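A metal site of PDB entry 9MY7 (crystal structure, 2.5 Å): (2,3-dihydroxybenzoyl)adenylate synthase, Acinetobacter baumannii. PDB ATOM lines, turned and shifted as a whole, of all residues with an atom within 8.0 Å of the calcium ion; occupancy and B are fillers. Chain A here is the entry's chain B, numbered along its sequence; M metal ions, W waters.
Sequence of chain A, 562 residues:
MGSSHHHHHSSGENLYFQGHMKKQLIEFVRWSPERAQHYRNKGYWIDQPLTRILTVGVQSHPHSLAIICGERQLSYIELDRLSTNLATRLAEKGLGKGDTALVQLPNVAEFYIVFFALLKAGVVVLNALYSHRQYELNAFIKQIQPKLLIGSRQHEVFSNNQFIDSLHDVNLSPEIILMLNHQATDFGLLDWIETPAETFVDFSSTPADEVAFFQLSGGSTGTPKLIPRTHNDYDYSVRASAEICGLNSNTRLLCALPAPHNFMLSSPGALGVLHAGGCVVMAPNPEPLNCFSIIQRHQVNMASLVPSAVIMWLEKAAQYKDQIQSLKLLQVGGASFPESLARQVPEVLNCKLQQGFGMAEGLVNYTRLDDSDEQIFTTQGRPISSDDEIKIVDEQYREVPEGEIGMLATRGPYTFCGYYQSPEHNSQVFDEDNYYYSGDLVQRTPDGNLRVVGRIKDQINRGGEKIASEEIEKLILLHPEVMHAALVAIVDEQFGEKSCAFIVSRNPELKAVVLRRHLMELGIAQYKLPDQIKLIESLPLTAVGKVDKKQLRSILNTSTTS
The calcium ion is bound by O of Asn 350 (2.3 Å), O of Gln 325 (2.4 Å), O of Leu 327 (2.4 Å) and water W1 (2.5 Å).
Three residues have an atom within 4 Å of the calcium ion: Gln 325, Leu 327 and Asn 350.
Water W1 lies within hydrogen-bond range of O of Leu 349 and N of Leu 327.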
ATOM      1  N   VAL A 300       2.753   6.366   9.934  1.00  0.00           N
ATOM      2  CA  VAL A 300       2.361   5.875   8.612  1.00  0.00           C
ATOM      3  C   VAL A 300       1.571   4.591   8.760  1.00  0.00           C
ATOM      4  O   VAL A 300       2.011   3.661   9.443  1.00  0.00           O
ATOM      5  CB  VAL A 300       3.608   5.676   7.734  1.00  0.00           C
ATOM      6  CG1 VAL A 300       3.236   4.977   6.433  1.00  0.00           C
ATOM      7  CG2 VAL A 300       4.298   7.004   7.461  1.00  0.00           C
ATOM      8  N   ASN A 301       0.402   4.529   8.134  1.00  0.00           N
ATOM      9  CA  ASN A 301      -0.443   3.346   8.210  1.00  0.00           C
ATOM     10  C   ASN A 301      -0.593   2.631   6.874  1.00  0.00           C
ATOM     11  O   ASN A 301      -1.385   1.685   6.772  1.00  0.00           O
ATOM     12  CB  ASN A 301      -1.830   3.698   8.771  1.00  0.00           C
ATOM     13  CG  ASN A 301      -2.494   4.830   8.004  1.00  0.00           C
ATOM     14  OD1 ASN A 301      -2.332   4.957   6.789  1.00  0.00           O
ATOM     15  ND2 ASN A 301      -3.269   5.639   8.711  1.00  0.00           N
ATOM     16  N   LYS A 321      10.061  -4.192  15.227  1.00  0.00           N
ATOM     17  CA  LYS A 321       8.609  -4.411  15.186  1.00  0.00           C
ATOM     18  C   LYS A 321       7.839  -3.187  15.665  1.00  0.00           C
ATOM     19  O   LYS A 321       6.771  -2.864  15.130  1.00  0.00           O
ATOM     20  CB  LYS A 321       8.244  -5.631  16.038  1.00  0.00           C
ATOM     21  CG  LYS A 321       8.290  -6.953  15.287  1.00  0.00           C
ATOM     22  CD  LYS A 321       7.859  -8.103  16.192  1.00  0.00           C
ATOM     23  N   ILE A 324       7.253  -0.011  13.281  1.00  0.00           N
ATOM     24  CA  ILE A 324       6.385  -0.222  12.132  1.00  0.00           C
ATOM     25  C   ILE A 324       5.033  -0.802  12.535  1.00  0.00           C
ATOM     26  O   ILE A 324       4.302  -1.301  11.680  1.00  0.00           O
ATOM     27  CB  ILE A 324       7.076  -1.110  11.076  1.00  0.00           C
ATOM     28  CG1 ILE A 324       7.383  -2.487  11.667  1.00  0.00           C
ATOM     29  CG2 ILE A 324       8.350  -0.451  10.576  1.00  0.00           C
ATOM     30  CD1 ILE A 324       7.464  -3.591  10.628  1.00  0.00           C
ATOM     31  N   GLN A 325       4.689  -0.748  13.826  1.00  0.00           N
ATOM     32  CA  GLN A 325       3.407  -1.266  14.274  1.00  0.00           C
ATOM     33  C   GLN A 325       2.244  -0.648  13.494  1.00  0.00           C
ATOM     34  O   GLN A 325       1.301  -1.340  13.117  1.00  0.00           O
ATOM     35  CB  GLN A 325       3.224  -1.004  15.771  1.00  0.00           C
ATOM     36  CG  GLN A 325       3.912  -1.981  16.723  1.00  0.00           C
ATOM     37  CD  GLN A 325       3.674  -3.449  16.390  1.00  0.00           C
ATOM     38  OE1 GLN A 325       3.100  -3.782  15.347  1.00  0.00           O
ATOM     39  NE2 GLN A 325       4.104  -4.333  17.284  1.00  0.00           N
ATOM     40  N   SER A 326       2.315   0.664  13.237  1.00  0.00           N
ATOM     41  CA  SER A 326       1.183   1.395  12.691  1.00  0.00           C
ATOM     42  C   SER A 326       0.852   1.004  11.257  1.00  0.00           C
ATOM     43  O   SER A 326      -0.238   1.367  10.780  1.00  0.00           O
ATOM     44  CB  SER A 326       1.448   2.905  12.756  1.00  0.00           C
ATOM     45  OG  SER A 326       2.346   3.312  11.746  1.00  0.00           O
ATOM     46  N   LEU A 327       1.724   0.294  10.561  1.00  0.00           N
ATOM     47  CA  LEU A 327       1.412  -0.162   9.218  1.00  0.00           C
ATOM     48  C   LEU A 327       0.142  -1.010   9.234  1.00  0.00           C
ATOM     49  O   LEU A 327      -0.004  -1.916  10.061  1.00  0.00           O
ATOM     50  CB  LEU A 327       2.574  -0.967   8.632  1.00  0.00           C
ATOM     51  CG  LEU A 327       3.513  -0.238   7.677  1.00  0.00           C
ATOM     52  CD1 LEU A 327       4.510  -1.199   7.065  1.00  0.00           C
ATOM     53  CD2 LEU A 327       2.723   0.481   6.595  1.00  0.00           C
ATOM     54  N   LYS A 328      -0.784  -0.696   8.328  1.00  0.00           N
ATOM     55  CA  LYS A 328      -2.036  -1.427   8.228  1.00  0.00           C
ATOM     56  C   LYS A 328      -2.208  -2.177   6.920  1.00  0.00           C
ATOM     57  O   LYS A 328      -2.889  -3.211   6.901  1.00  0.00           O
ATOM     58  CB  LYS A 328      -3.236  -0.480   8.410  1.00  0.00           C
ATOM     59  CG  LYS A 328      -3.504  -0.065   9.846  1.00  0.00           C
ATOM     60  CD  LYS A 328      -4.757   0.790   9.951  1.00  0.00           C
ATOM     61  CE  LYS A 328      -4.564   1.940  10.922  1.00  0.00           C
ATOM     62  NZ  LYS A 328      -3.302   1.818  11.700  1.00  0.00           N
ATOM     63  N   LEU A 329      -1.610  -1.701   5.826  1.00  0.00           N
ATOM     64  CA  LEU A 329      -1.793  -2.324   4.525  1.00  0.00           C
ATOM     65  C   LEU A 329      -0.549  -2.075   3.683  1.00  0.00           C
ATOM     66  O   LEU A 329      -0.011  -0.956   3.671  1.00  0.00           O
ATOM     67  CB  LEU A 329      -3.029  -1.768   3.815  1.00  0.00           C
ATOM     68  CG  LEU A 329      -3.351  -2.305   2.421  1.00  0.00           C
ATOM     69  CD1 LEU A 329      -3.628  -3.794   2.470  1.00  0.00           C
ATOM     70  CD2 LEU A 329      -4.533  -1.561   1.824  1.00  0.00           C
ATOM     71  N   PRO A 346       2.257 -10.397   6.330  1.00  0.00           N
ATOM     72  CA  PRO A 346       1.454 -10.277   7.563  1.00  0.00           C
ATOM     73  C   PRO A 346       2.189 -10.756   8.800  1.00  0.00           C
ATOM     74  O   PRO A 346       2.059 -10.143   9.869  1.00  0.00           O
ATOM     75  CB  PRO A 346       0.211 -11.136   7.271  1.00  0.00           C
ATOM     76  CG  PRO A 346       0.566 -11.978   6.096  1.00  0.00           C
ATOM     77  CD  PRO A 346       1.614 -11.254   5.321  1.00  0.00           C
ATOM     78  N   LEU A 349       5.759  -8.180   9.038  1.00  0.00           N
ATOM     79  CA  LEU A 349       5.483  -6.746   8.984  1.00  0.00           C
ATOM     80  C   LEU A 349       4.202  -6.369   9.704  1.00  0.00           C
ATOM     81  O   LEU A 349       3.909  -5.172   9.818  1.00  0.00           O
ATOM     82  CB  LEU A 349       5.416  -6.286   7.528  1.00  0.00           C
ATOM     83  CG  LEU A 349       6.730  -6.420   6.734  1.00  0.00           C
ATOM     84  CD1 LEU A 349       6.535  -6.007   5.280  1.00  0.00           C
ATOM     85  CD2 LEU A 349       7.832  -5.602   7.388  1.00  0.00           C
ATOM     86  N   ASN A 350       3.430  -7.339  10.202  1.00  0.00           N
ATOM     87  CA  ASN A 350       2.252  -7.088  11.028  1.00  0.00           C
ATOM     88  C   ASN A 350       1.280  -6.143  10.321  1.00  0.00           C
ATOM     89  O   ASN A 350       0.971  -5.048  10.792  1.00  0.00           O
ATOM     90  CB  ASN A 350       2.660  -6.528  12.393  1.00  0.00           C
ATOM     91  CG  ASN A 350       3.825  -7.283  13.000  1.00  0.00           C
ATOM     92  OD1 ASN A 350       3.980  -8.482  12.799  1.00  0.00           O
ATOM     93  ND2 ASN A 350       4.665  -6.571  13.756  1.00  0.00           N
ATOM     94  N   CYS A 351       0.782  -6.597   9.170  1.00  0.00           N
ATOM     95  CA  CYS A 351      -0.074  -5.752   8.351  1.00  0.00           C
ATOM     96  C   CYS A 351      -0.699  -6.602   7.241  1.00  0.00           C
ATOM     97  O   CYS A 351      -0.205  -7.673   6.900  1.00  0.00           O
ATOM     98  CB  CYS A 351       0.703  -4.582   7.746  1.00  0.00           C
ATOM     99  SG  CYS A 351       1.527  -4.969   6.179  1.00  0.00           S
ATOM    100  N   LYS A 352      -1.808  -6.098   6.701  1.00  0.00           N
ATOM    101  CA  LYS A 352      -2.474  -6.761   5.599  1.00  0.00           C
ATOM    102  C   LYS A 352      -1.664  -6.644   4.322  1.00  0.00           C
ATOM    103  O   LYS A 352      -0.897  -5.689   4.131  1.00  0.00           O
ATOM    104  CB  LYS A 352      -3.873  -6.162   5.383  1.00  0.00           C
ATOM    105  CG  LYS A 352      -4.757  -6.943   4.418  1.00  0.00           C
ATOM    106  CD  LYS A 352      -5.058  -8.343   4.913  1.00  0.00           C
ATOM    107  CE  LYS A 352      -5.105  -9.337   3.756  1.00  0.00           C
ATOM    108  NZ  LYS A 352      -4.525 -10.658   4.135  1.00  0.00           N
HETATM  109 CA    CA M   1       0.355  -3.246  12.053  1.00  0.00          CA
HETATM  110  O   HOH W   1       2.708  -2.893  11.340  1.00  0.00           O
